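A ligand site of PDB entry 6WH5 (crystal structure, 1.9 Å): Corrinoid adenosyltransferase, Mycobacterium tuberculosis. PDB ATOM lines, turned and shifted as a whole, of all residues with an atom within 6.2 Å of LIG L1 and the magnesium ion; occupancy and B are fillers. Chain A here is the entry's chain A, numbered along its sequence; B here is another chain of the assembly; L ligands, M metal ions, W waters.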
ATOM      1  N   ILE A  11      -7.170 -28.942 -33.481  1.00  0.00           N
ATOM      2  CA  ILE A  11      -8.053 -27.783 -33.491  1.00  0.00           C
ATOM      3  C   ILE A  11      -9.528 -28.148 -33.311  1.00  0.00           C
ATOM      4  O   ILE A  11     -10.163 -27.692 -32.365  1.00  0.00           O
ATOM      5  CB  ILE A  11      -7.901 -26.907 -34.758  1.00  0.00           C
ATOM      6  CG1 ILE A  11      -6.432 -26.591 -35.037  1.00  0.00           C
ATOM      7  CG2 ILE A  11      -8.684 -25.595 -34.582  1.00  0.00           C
ATOM      8  CD1 ILE A  11      -5.688 -25.986 -33.862  1.00  0.00           C
ATOM      9  N   TYR A  12     -10.104 -28.924 -34.229  1.00  0.00           N
ATOM     10  CA  TYR A  12     -11.513 -29.300 -34.087  1.00  0.00           C
ATOM     11  C   TYR A  12     -11.640 -30.571 -33.254  1.00  0.00           C
ATOM     12  O   TYR A  12     -11.036 -31.594 -33.585  1.00  0.00           O
ATOM     13  CB  TYR A  12     -12.214 -29.461 -35.440  1.00  0.00           C
ATOM     14  CG  TYR A  12     -11.862 -30.664 -36.294  1.00  0.00           C
ATOM     15  CD1 TYR A  12     -12.607 -31.836 -36.221  1.00  0.00           C
ATOM     16  CD2 TYR A  12     -10.812 -30.607 -37.211  1.00  0.00           C
ATOM     17  CE1 TYR A  12     -12.306 -32.927 -37.017  1.00  0.00           C
ATOM     18  CE2 TYR A  12     -10.499 -31.693 -38.006  1.00  0.00           C
ATOM     19  CZ  TYR A  12     -11.258 -32.847 -37.913  1.00  0.00           C
ATOM     20  OH  TYR A  12     -10.952 -33.936 -38.701  1.00  0.00           O
ATOM     21  N   THR A  13     -12.423 -30.493 -32.174  1.00  0.00           N
ATOM     22  CA  THR A  13     -12.668 -31.634 -31.289  1.00  0.00           C
ATOM     23  C   THR A  13     -14.120 -32.096 -31.296  1.00  0.00           C
ATOM     24  O   THR A  13     -14.396 -33.207 -30.839  1.00  0.00           O
ATOM     25  CB  THR A  13     -12.293 -31.277 -29.841  1.00  0.00           C
ATOM     26  OG1 THR A  13     -13.318 -30.459 -29.264  1.00  0.00           O
ATOM     27  CG2 THR A  13     -10.960 -30.537 -29.793  1.00  0.00           C
ATOM     28  N   ARG A  14     -15.047 -31.275 -31.797  1.00  0.00           N
ATOM     29  CA  ARG A  14     -16.483 -31.543 -31.857  1.00  0.00           C
ATOM     30  C   ARG A  14     -17.145 -31.576 -30.490  1.00  0.00           C
ATOM     31  O   ARG A  14     -18.367 -31.834 -30.408  1.00  0.00           O
ATOM     32  CB  ARG A  14     -16.796 -32.864 -32.588  1.00  0.00           C
ATOM     33  CG  ARG A  14     -16.068 -33.039 -33.925  1.00  0.00           C
ATOM     34  CD  ARG A  14     -16.769 -34.081 -34.781  1.00  0.00           C
ATOM     35  NE  ARG A  14     -16.024 -34.467 -35.991  1.00  0.00           N
ATOM     36  CZ  ARG A  14     -15.242 -35.541 -36.089  1.00  0.00           C
ATOM     37  NH1 ARG A  14     -15.065 -36.352 -35.049  1.00  0.00           N
ATOM     38  NH2 ARG A  14     -14.625 -35.811 -37.232  1.00  0.00           N
ATOM     39  N   THR A  15     -16.421 -31.313 -29.406  1.00  0.00           N
ATOM     40  CA  THR A  15     -17.055 -31.329 -28.094  1.00  0.00           C
ATOM     41  C   THR A  15     -17.968 -30.125 -27.866  1.00  0.00           C
ATOM     42  O   THR A  15     -18.663 -30.071 -26.851  1.00  0.00           O
ATOM     43  CB  THR A  15     -15.999 -31.381 -26.987  1.00  0.00           C
ATOM     44  OG1 THR A  15     -15.130 -30.239 -27.058  1.00  0.00           O
ATOM     45  CG2 THR A  15     -15.171 -32.633 -27.141  1.00  0.00           C
ATOM     46  N   GLY A  16     -17.983 -29.154 -28.785  1.00  0.00           N
ATOM     47  CA  GLY A  16     -18.880 -28.028 -28.718  1.00  0.00           C
ATOM     48  C   GLY A  16     -20.095 -28.130 -29.626  1.00  0.00           C
ATOM     49  O   GLY A  16     -20.845 -27.151 -29.750  1.00  0.00           O
ATOM     50  N   ASP A  17     -20.302 -29.281 -30.276  1.00  0.00           N
ATOM     51  CA  ASP A  17     -21.365 -29.458 -31.243  1.00  0.00           C
ATOM     52  C   ASP A  17     -22.756 -29.547 -30.610  1.00  0.00           C
ATOM     53  O   ASP A  17     -23.739 -29.588 -31.341  1.00  0.00           O
ATOM     54  CB  ASP A  17     -21.107 -30.716 -32.079  1.00  0.00           C
ATOM     55  CG  ASP A  17     -20.040 -30.521 -33.141  1.00  0.00           C
ATOM     56  OD1 ASP A  17     -19.621 -29.359 -33.384  1.00  0.00           O
ATOM     57  OD2 ASP A  17     -19.619 -31.537 -33.739  1.00  0.00           O
ATOM     58  N   THR A  20     -22.479 -26.363 -25.980  1.00  0.00           N
ATOM     59  CA  THR A  20     -21.796 -26.117 -24.722  1.00  0.00           C
ATOM     60  C   THR A  20     -20.304 -26.037 -24.979  1.00  0.00           C
ATOM     61  O   THR A  20     -19.797 -26.500 -26.004  1.00  0.00           O
ATOM     62  CB  THR A  20     -22.089 -27.215 -23.678  1.00  0.00           C
ATOM     63  OG1 THR A  20     -21.415 -28.426 -24.042  1.00  0.00           O
ATOM     64  CG2 THR A  20     -23.571 -27.490 -23.550  1.00  0.00           C
ATOM     65  N   THR A  21     -19.583 -25.431 -24.039  1.00  0.00           N
ATOM     66  CA  THR A  21     -18.128 -25.334 -24.136  1.00  0.00           C
ATOM     67  C   THR A  21     -17.570 -25.350 -22.724  1.00  0.00           C
ATOM     68  O   THR A  21     -18.295 -25.521 -21.739  1.00  0.00           O
ATOM     69  CB  THR A  21     -17.728 -24.091 -24.957  1.00  0.00           C
ATOM     70  OG1 THR A  21     -16.362 -24.214 -25.387  1.00  0.00           O
ATOM     71  CG2 THR A  21     -17.897 -22.803 -24.165  1.00  0.00           C
ATOM     72  N   GLY A  22     -16.248 -25.228 -22.625  1.00  0.00           N
ATOM     73  CA  GLY A  22     -15.547 -25.423 -21.375  1.00  0.00           C
ATOM     74  C   GLY A  22     -14.814 -24.177 -20.926  1.00  0.00           C
ATOM     75  O   GLY A  22     -14.159 -23.511 -21.729  1.00  0.00           O
ATOM     76  N   ARG A  28     -18.453 -26.915 -17.581  1.00  0.00           N
ATOM     77  CA  ARG A  28     -19.201 -26.737 -18.827  1.00  0.00           C
ATOM     78  C   ARG A  28     -20.176 -25.572 -18.709  1.00  0.00           C
ATOM     79  O   ARG A  28     -20.789 -25.359 -17.656  1.00  0.00           O
ATOM     80  CB  ARG A  28     -19.967 -28.012 -19.185  1.00  0.00           C
ATOM     81  CG  ARG A  28     -19.091 -29.263 -19.258  1.00  0.00           C
ATOM     82  CD  ARG A  28     -18.015 -29.151 -20.338  1.00  0.00           C
ATOM     83  NE  ARG A  28     -18.610 -29.027 -21.663  1.00  0.00           N
ATOM     84  CZ  ARG A  28     -17.916 -28.832 -22.778  1.00  0.00           C
ATOM     85  NH1 ARG A  28     -16.596 -28.735 -22.749  1.00  0.00           N
ATOM     86  NH2 ARG A  28     -18.546 -28.723 -23.935  1.00  0.00           N
ATOM     87  N   LYS A  31     -22.941 -21.974 -24.698  1.00  0.00           N
ATOM     88  CA  LYS A  31     -22.181 -21.071 -25.564  1.00  0.00           C
ATOM     89  C   LYS A  31     -22.779 -19.672 -25.626  1.00  0.00           C
ATOM     90  O   LYS A  31     -22.271 -18.822 -26.358  1.00  0.00           O
ATOM     91  CB  LYS A  31     -22.065 -21.663 -26.973  1.00  0.00           C
ATOM     92  CG  LYS A  31     -20.858 -22.595 -27.110  1.00  0.00           C
ATOM     93  CD  LYS A  31     -20.703 -23.173 -28.503  1.00  0.00           C
ATOM     94  CE  LYS A  31     -19.451 -24.024 -28.611  1.00  0.00           C
ATOM     95  NZ  LYS A  31     -19.322 -24.755 -29.902  1.00  0.00           N
ATOM     96  N   ARG B 140     -17.209 -16.913 -34.924  1.00  0.00           N
ATOM     97  CA  ARG B 140     -17.489 -17.428 -33.597  1.00  0.00           C
ATOM     98  C   ARG B 140     -18.622 -16.656 -32.941  1.00  0.00           C
ATOM     99  O   ARG B 140     -19.466 -17.237 -32.266  1.00  0.00           O
ATOM    100  CB  ARG B 140     -16.225 -17.407 -32.755  1.00  0.00           C
ATOM    101  CG  ARG B 140     -15.258 -18.496 -33.216  1.00  0.00           C
ATOM    102  CD  ARG B 140     -13.885 -18.343 -32.632  1.00  0.00           C
ATOM    103  NE  ARG B 140     -13.840 -18.768 -31.243  1.00  0.00           N
ATOM    104  CZ  ARG B 140     -13.820 -20.040 -30.841  1.00  0.00           C
ATOM    105  NH1 ARG B 140     -13.855 -21.044 -31.725  1.00  0.00           N
ATOM    106  NH2 ARG B 140     -13.780 -20.312 -29.541  1.00  0.00           N
ATOM    107  N   GLU B 143     -21.731 -18.047 -34.423  1.00  0.00           N
ATOM    108  CA  GLU B 143     -22.074 -19.346 -33.846  1.00  0.00           C
ATOM    109  C   GLU B 143     -22.862 -19.184 -32.563  1.00  0.00           C
ATOM    110  O   GLU B 143     -23.855 -19.885 -32.341  1.00  0.00           O
ATOM    111  CB  GLU B 143     -20.808 -20.151 -33.564  1.00  0.00           C
ATOM    112  CG  GLU B 143     -21.105 -21.617 -33.248  1.00  0.00           C
ATOM    113  CD  GLU B 143     -20.018 -22.268 -32.415  1.00  0.00           C
ATOM    114  OE1 GLU B 143     -18.889 -21.730 -32.396  1.00  0.00           O
ATOM    115  OE2 GLU B 143     -20.300 -23.308 -31.790  1.00  0.00           O
ATOM    116  N   ASN B 166     -19.429 -23.713 -36.004  1.00  0.00           N
ATOM    117  CA  ASN B 166     -18.431 -24.199 -35.060  1.00  0.00           C
ATOM    118  C   ASN B 166     -17.185 -24.688 -35.787  1.00  0.00           C
ATOM    119  O   ASN B 166     -16.076 -24.241 -35.505  1.00  0.00           O
ATOM    120  CB  ASN B 166     -19.032 -25.310 -34.200  1.00  0.00           C
ATOM    121  CG  ASN B 166     -18.129 -25.692 -33.038  1.00  0.00           C
ATOM    122  OD1 ASN B 166     -17.366 -24.869 -32.533  1.00  0.00           O
ATOM    123  ND2 ASN B 166     -18.216 -26.948 -32.608  1.00  0.00           N
ATOM    124  N   ARG B 167     -17.364 -25.620 -36.739  1.00  0.00           N
ATOM    125  CA  ARG B 167     -16.205 -26.142 -37.464  1.00  0.00           C
ATOM    126  C   ARG B 167     -15.541 -25.060 -38.312  1.00  0.00           C
ATOM    127  O   ARG B 167     -14.319 -25.095 -38.507  1.00  0.00           O
ATOM    128  CB  ARG B 167     -16.633 -27.330 -38.334  1.00  0.00           C
ATOM    129  CG  ARG B 167     -15.536 -28.360 -38.561  1.00  0.00           C
ATOM    130  CD  ARG B 167     -15.274 -29.193 -37.303  1.00  0.00           C
ATOM    131  NE  ARG B 167     -16.296 -30.224 -37.103  1.00  0.00           N
ATOM    132  CZ  ARG B 167     -17.240 -30.200 -36.167  1.00  0.00           C
ATOM    133  NH1 ARG B 167     -17.324 -29.197 -35.291  1.00  0.00           N
ATOM    134  NH2 ARG B 167     -18.110 -31.193 -36.093  1.00  0.00           N
ATOM    135  N   SER B 169     -14.919 -21.848 -37.786  1.00  0.00           N
ATOM    136  CA  SER B 169     -13.938 -20.982 -37.141  1.00  0.00           C
ATOM    137  C   SER B 169     -12.632 -21.731 -36.886  1.00  0.00           C
ATOM    138  O   SER B 169     -11.562 -21.109 -36.887  1.00  0.00           O
ATOM    139  CB  SER B 169     -14.514 -20.391 -35.847  1.00  0.00           C
ATOM    140  OG  SER B 169     -14.632 -21.329 -34.789  1.00  0.00           O
ATOM    141  N   ASP B 170     -12.690 -23.042 -36.714  1.00  0.00           N
ATOM    142  CA  ASP B 170     -11.475 -23.844 -36.634  1.00  0.00           C
ATOM    143  C   ASP B 170     -10.712 -23.825 -37.959  1.00  0.00           C
ATOM    144  O   ASP B 170      -9.476 -23.698 -37.979  1.00  0.00           O
ATOM    145  CB  ASP B 170     -11.811 -25.277 -36.244  1.00  0.00           C
ATOM    146  CG  ASP B 170     -12.243 -25.415 -34.788  1.00  0.00           C
ATOM    147  OD1 ASP B 170     -12.108 -24.443 -34.002  1.00  0.00           O
ATOM    148  OD2 ASP B 170     -12.724 -26.508 -34.423  1.00  0.00           O
HETATM  149  P1  LIG L   1     -15.107 -27.560 -30.733  1.00  0.00           P
HETATM  150  O1  LIG L   1     -15.015 -26.403 -31.686  1.00  0.00           O
HETATM  151  O2  LIG L   1     -16.330 -28.466 -30.841  1.00  0.00           O
HETATM  152  O3  LIG L   1     -13.935 -28.554 -30.779  1.00  0.00           O
HETATM  153  P2  LIG L   1     -15.628 -25.831 -28.565  1.00  0.00           P
HETATM  154  O4  LIG L   1     -16.673 -25.332 -29.555  1.00  0.00           O
HETATM  155  O5  LIG L   1     -16.397 -26.077 -27.263  1.00  0.00           O
HETATM  156  O6  LIG L   1     -15.149 -27.219 -29.136  1.00  0.00           O
HETATM  157  P3  LIG L   1     -13.215 -23.956 -29.218  1.00  0.00           P
HETATM  158  O7  LIG L   1     -12.069 -24.926 -29.224  1.00  0.00           O
HETATM  159  O8  LIG L   1     -13.173 -22.746 -28.318  1.00  0.00           O
HETATM  160  O9  LIG L   1     -14.467 -24.895 -28.484  1.00  0.00           O
HETATM  161  O10 LIG L   1     -13.861 -23.747 -30.585  1.00  0.00           O
HETATM  162 CO1  LG2 L   2      -9.213 -21.986 -26.876  1.00  0.00          CO
HETATM  163  N1  LG2 L   2      -8.813 -23.774 -27.201  1.00  0.00           N
HETATM  164  N2  LG2 L   2      -9.111 -21.638 -28.764  1.00  0.00           N
HETATM  165  N3  LG2 L   2      -9.719 -20.290 -26.350  1.00  0.00           N
HETATM  166  N4  LG2 L   2      -9.247 -22.569 -25.070  1.00  0.00           N
HETATM  167  C1  LG2 L   2      -8.436 -24.656 -26.061  1.00  0.00           C
HETATM  168  C2  LG2 L   2      -6.893 -24.598 -25.854  1.00  0.00           C
HETATM  169  C3  LG2 L   2      -8.977 -26.098 -26.507  1.00  0.00           C
HETATM  170  C4  LG2 L   2      -8.221 -27.282 -25.831  1.00  0.00           C
HETATM  171  C5  LG2 L   2     -10.510 -26.172 -26.245  1.00  0.00           C
HETATM  172  C6  LG2 L   2     -11.165 -27.457 -26.759  1.00  0.00           C
HETATM  173  O1  LG2 L   2     -11.103 -28.558 -26.224  1.00  0.00           O
HETATM  174  N5  LG2 L   2     -11.883 -27.337 -27.888  1.00  0.00           N
HETATM  175  C7  LG2 L   2      -8.780 -25.965 -28.035  1.00  0.00           C
HETATM  176  C8  LG2 L   2      -7.521 -26.619 -28.729  1.00  0.00           C
HETATM  177  C9  LG2 L   2      -7.927 -28.027 -29.259  1.00  0.00           C
HETATM  178  C10 LG2 L   2      -6.812 -28.828 -29.930  1.00  0.00           C
HETATM  179  O2  LG2 L   2      -6.307 -28.398 -30.970  1.00  0.00           O
HETATM  180  N6  LG2 L   2      -6.341 -29.952 -29.416  1.00  0.00           N
HETATM  181  C11 LG2 L   2      -8.844 -24.468 -28.305  1.00  0.00           C
HETATM  182  C12 LG2 L   2      -8.905 -23.885 -29.628  1.00  0.00           C
HETATM  183  C13 LG2 L   2      -9.198 -24.859 -30.807  1.00  0.00           C
HETATM  184  C14 LG2 L   2      -8.945 -22.526 -29.829  1.00  0.00           C
HETATM  185  C15 LG2 L   2      -9.125 -21.784 -31.164  1.00  0.00           C
HETATM  186  C16 LG2 L   2      -8.293 -22.287 -32.351  1.00  0.00           C
HETATM  187  C17 LG2 L   2     -10.664 -21.750 -31.487  1.00  0.00           C
HETATM  188  C18 LG2 L   2     -10.878 -21.012 -32.846  1.00  0.00           C
HETATM  189  O3  LG2 L   2     -10.865 -19.750 -32.828  1.00  0.00           O
HETATM  190  N7  LG2 L   2     -11.074 -21.754 -33.917  1.00  0.00           N
HETATM  191  C19 LG2 L   2      -8.784 -20.329 -30.718  1.00  0.00           C
HETATM  192  C20 LG2 L   2      -7.264 -19.988 -30.874  1.00  0.00           C
HETATM  193  C21 LG2 L   2      -6.967 -18.559 -30.423  1.00  0.00           C
HETATM  194  C22 LG2 L   2      -5.682 -17.979 -30.898  1.00  0.00           C
HETATM  195  O4  LG2 L   2      -4.625 -18.662 -30.917  1.00  0.00           O
HETATM  196  N8  LG2 L   2      -5.603 -16.704 -31.315  1.00  0.00           N
HETATM  197  C23 LG2 L   2      -9.116 -20.396 -29.235  1.00  0.00           C
HETATM  198  C24 LG2 L   2      -9.626 -19.312 -28.560  1.00  0.00           C
HETATM  199  C25 LG2 L   2      -9.853 -19.253 -27.208  1.00  0.00           C
HETATM  200  C26 LG2 L   2     -10.093 -17.942 -26.499  1.00  0.00           C
HETATM  201  C27 LG2 L   2     -11.426 -17.378 -27.084  1.00  0.00           C
HETATM  202  C28 LG2 L   2      -8.954 -16.926 -26.790  1.00  0.00           C
HETATM  203  C29 LG2 L   2     -10.372 -18.396 -25.046  1.00  0.00           C
HETATM  204  C30 LG2 L   2      -9.599 -17.520 -23.975  1.00  0.00           C
HETATM  205  C31 LG2 L   2      -8.111 -17.872 -23.902  1.00  0.00           C
HETATM  206  C32 LG2 L   2      -7.287 -16.655 -23.411  1.00  0.00           C
HETATM  207  O5  LG2 L   2      -7.668 -15.491 -23.785  1.00  0.00           O
HETATM  208  N9  LG2 L   2      -6.268 -16.856 -22.665  1.00  0.00           N
HETATM  209  C33 LG2 L   2      -9.900 -19.833 -25.042  1.00  0.00           C
HETATM  210  C34 LG2 L   2     -10.121 -20.624 -23.909  1.00  0.00           C
HETATM  211  C35 LG2 L   2     -10.824 -20.071 -22.658  1.00  0.00           C
HETATM  212  C36 LG2 L   2      -9.746 -22.005 -24.019  1.00  0.00           C
HETATM  213  C37 LG2 L   2      -9.240 -22.858 -22.808  1.00  0.00           C
HETATM  214  C38 LG2 L   2     -10.659 -23.181 -22.178  1.00  0.00           C
HETATM  215  C39 LG2 L   2      -8.374 -22.258 -21.745  1.00  0.00           C
HETATM  216  C40 LG2 L   2      -7.042 -21.819 -22.412  1.00  0.00           C
HETATM  217  C41 LG2 L   2      -6.250 -20.818 -21.548  1.00  0.00           C
HETATM  218  O6  LG2 L   2      -6.456 -19.620 -21.649  1.00  0.00           O
HETATM  219  N10 LG2 L   2      -5.321 -21.337 -20.764  1.00  0.00           N
HETATM  220  C42 LG2 L   2      -8.704 -24.165 -23.440  1.00  0.00           C
HETATM  221  C43 LG2 L   2      -9.098 -25.569 -22.892  1.00  0.00           C
HETATM  222  C44 LG2 L   2      -8.270 -25.921 -21.665  1.00  0.00           C
HETATM  223  O7  LG2 L   2      -7.029 -25.846 -21.698  1.00  0.00           O
HETATM  224  N11 LG2 L   2      -8.966 -26.290 -20.596  1.00  0.00           N
HETATM  225  C45 LG2 L   2      -9.213 -24.015 -24.860  1.00  0.00           C
HETATM  226  C46 LG2 L   2      -4.551 -20.349 -19.987  1.00  0.00           C
HETATM  227  C47 LG2 L   2      -4.508 -20.717 -18.507  1.00  0.00           C
HETATM  228  C48 LG2 L   2      -5.842 -20.432 -17.823  1.00  0.00           C
HETATM  229  O8  LG2 L   2      -4.243 -22.153 -18.467  1.00  0.00           O
HETATM  230  O9  LG2 L   2      -3.480 -24.060 -16.992  1.00  0.00           O
HETATM  231  O10 LG2 L   2      -1.746 -22.546 -18.220  1.00  0.00           O
HETATM  232  P1  LG2 L   2      -3.088 -22.741 -17.510  1.00  0.00           P
HETATM  233  O11 LG2 L   2      -3.069 -21.641 -16.296  1.00  0.00           O
HETATM  234  C49 LG2 L   2      -2.914 -22.084 -14.992  1.00  0.00           C
HETATM  235  C50 LG2 L   2      -1.579 -21.991 -14.274  1.00  0.00           C
HETATM  236  O12 LG2 L   2      -0.485 -22.502 -14.975  1.00  0.00           O
HETATM  237  C51 LG2 L   2      -1.487 -20.452 -13.974  1.00  0.00           C
HETATM  238  O13 LG2 L   2      -2.793 -19.965 -14.152  1.00  0.00           O
HETATM  239  C52 LG2 L   2      -3.735 -21.062 -14.144  1.00  0.00           C
HETATM  240  C53 LG2 L   2      -4.083 -21.566 -12.750  1.00  0.00           C
HETATM  241  O14 LG2 L   2      -5.544 -21.567 -12.628  1.00  0.00           O
HETATM  242  N12 LG2 L   2      -0.572 -19.684 -14.841  1.00  0.00           N
HETATM  243  C54 LG2 L   2       0.003 -18.459 -14.522  1.00  0.00           C
HETATM  244  C55 LG2 L   2      -0.101 -20.021 -16.055  1.00  0.00           C
HETATM  245  N13 LG2 L   2       0.718 -19.110 -16.542  1.00  0.00           N
HETATM  246  C56 LG2 L   2       0.805 -18.094 -15.584  1.00  0.00           C
HETATM  247  C57 LG2 L   2       1.512 -16.878 -15.547  1.00  0.00           C
HETATM  248  C58 LG2 L   2       1.348 -16.092 -14.394  1.00  0.00           C
HETATM  249  C59 LG2 L   2       2.063 -14.771 -14.238  1.00  0.00           C
HETATM  250  C60 LG2 L   2       0.499 -16.482 -13.271  1.00  0.00           C
HETATM  251  C61 LG2 L   2       0.374 -15.605 -12.075  1.00  0.00           C
HETATM  252  C62 LG2 L   2      -0.189 -17.704 -13.349  1.00  0.00           C
HETATM  253 MG    MG M   1     -15.629 -24.451 -31.429  1.00  0.00          MG
HETATM  254  O   HOH W   1     -14.622 -23.881 -33.298  1.00  0.00           O
HETATM  255  O   HOH W   2     -13.592 -20.169 -26.101  1.00  0.00           O
HETATM  256  O   HOH W   3     -12.262 -22.678 -26.083  1.00  0.00           O
HETATM  257  O   HOH W   4     -16.676 -22.651 -31.070  1.00  0.00           O
HETATM  258  O   HOH W   5     -15.165 -27.410 -34.371  1.00  0.00           O
HETATM  259  O   HOH W   6     -16.036 -28.284 -25.673  1.00  0.00           O
HETATM  260  O   HOH W   7     -15.430 -22.050 -26.770  1.00  0.00           O
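The backbone NH (N) of Thr 13 lies within hydrogen-bond range of an oxygen (O3) of LIG L1 (2.8 Å). OG1 of Thr 13 lies within hydrogen-bond range of O3 of LIG L1 (2.5 Å). O5 of LIG L1 lies within hydrogen-bond range of OG1 of Thr 21, at 2.6 Å. The backbone NH (N) of Gly 16 lies within hydrogen-bond range of an oxygen (O2) of LIG L1 (2.7 Å). The side-chain amino group of Lys 31 lies close to an oxygen (O4) of LIG L1, 2.7 Å away. NH2 of Arg 140 of chain B is in salt-bridge range of O8 of LIG L1. O3 of LIG L1 lies within hydrogen-bond range of N of Arg 14 (3.1 Å). O2 of LIG L1 is in hydrogen-bond range of N of Thr 15 (3.2 Å). NH1 of Arg 140 of chain B sits close to O3 of LG2 L2 (3.4 Å). The side-chain carboxylate of Asp 170 of chain B is in hydrogen-bond range of a nitrogen (N7) of LG2 L2 (2.9 Å). An oxygen (O2) of LG2 L2 is in hydrogen-bond range of the backbone NH of Ile 11 (2.7 Å). A nitrogen (N7) of LG2 L2 lies within hydrogen-bond range of the backbone carbonyl oxygen of Ser 169 of chain B (3.1 Å).
A nitrogen (N5) of LG2 L2 sits at hydrogen-bond distance from an oxygen (O7) of LIG L1.
The side-chain amide oxygen (OD1) of Asn 166 of chain B lies close to the side-chain amino group (NZ) of Lys 31, 3.3 Å away. The side-chain carboxylate of Asp 17 is in hydrogen-bond range of the side-chain amide nitrogen of Asn 166 of chain B (2.9 Å). OD1 of Asn 166 of chain B sits close to OE2 of Glu 143 of chain B, 3.4 Å away. OG1 of Thr 15 lies within hydrogen-bond range of OG1 of Thr 13 (2.9 Å). The side-chain amino group (NZ) of Lys 31 sits at hydrogen-bond distance from the backbone carbonyl oxygen (O) of Gly 16, 2.8 Å away. The side-chain amino group (NZ) of Lys 31 is in salt-bridge range of the side-chain carboxylate (OE2) of Glu 143 of chain B (2.6 Å). The side-chain hydroxyl (OG) of Ser 169 of chain B is in hydrogen-bond range of the guanidinium group (NH1) of Arg 140 of chain B. O of Thr 15 is in hydrogen-bond range of NH2 of Arg 28, 3.2 Å away.
Tyr 12 touches LIG L1 (C to O3, 3.9 Å). Thr 20 touches LIG L1 (O to O5, 3.7 Å). OD2 of Asp 170 of chain B touches O1 of LIG L1, at 3.6 Å. Within 4 Å of LIG L1: Tyr 12, Thr 13, Arg 14, Thr 15, Gly 16, Thr 20, Thr 21, Lys 31, Arg 140 of chain B, Asn 166 of chain B and Asp 170 of chain B.
Merely in contact with the magnesium ion: Arg 140 of chain B. Within 4 Å of the magnesium ion: Arg 140 of chain B and Asn 166 of chain B. The nearest printed residue that does not touch the magnesium ion is Lys 31 (4.01 Å).
The magnesium ion is bound by an oxygen (O1) of LIG L1 (2.1 Å), an oxygen (O10) of LIG L1 (2.1 Å), the side-chain amide oxygen (OD1) of Asn 166 of chain B (2.1 Å), water W4 (2.1 Å), water W1 (2.2 Å) and an oxygen (O4) of LIG L1 (2.3 Å).
Water W1 lies within hydrogen-bond range of the backbone carbonyl oxygen of Asn 166 of chain B (2.7 Å), the side-chain carboxylate of Asp 170 of chain B (2.7 Å), the side-chain hydroxyl of Ser 169 of chain B (3.0 Å) and the guanidinium group of Arg 140 of chain B (3.3 Å). Water W4 lies within hydrogen-bond range of the side-chain carboxylate of Glu 143 of chain B (2.7 Å) and the guanidinium group of Arg 140 of chain B (3.3 Å). Water W6 lies within hydrogen-bond range of the side-chain hydroxyl (OG1) of Thr 15 (2.6 Å), an oxygen (O5) of LIG L1 (2.7 Å) and the guanidinium group (NH1) of Arg 28 (3.0 Å). Water W7 lies within hydrogen-bond range of the side-chain hydroxyl (OG1) of Thr 21 (2.7 Å) and an oxygen (O8) of LIG L1 (2.8 Å). Water W5 lies within hydrogen-bond range of OD2 of Asp 170 of chain B (2.6 Å), NH1 of Arg 167 of chain B (2.9 Å) and O of Asn 166 of chain B (3.5 Å). Water W2 lies within hydrogen-bond range of O8 of LIG L1 (3.4 Å) and NH2 of Arg 140 of chain B (3.4 Å).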
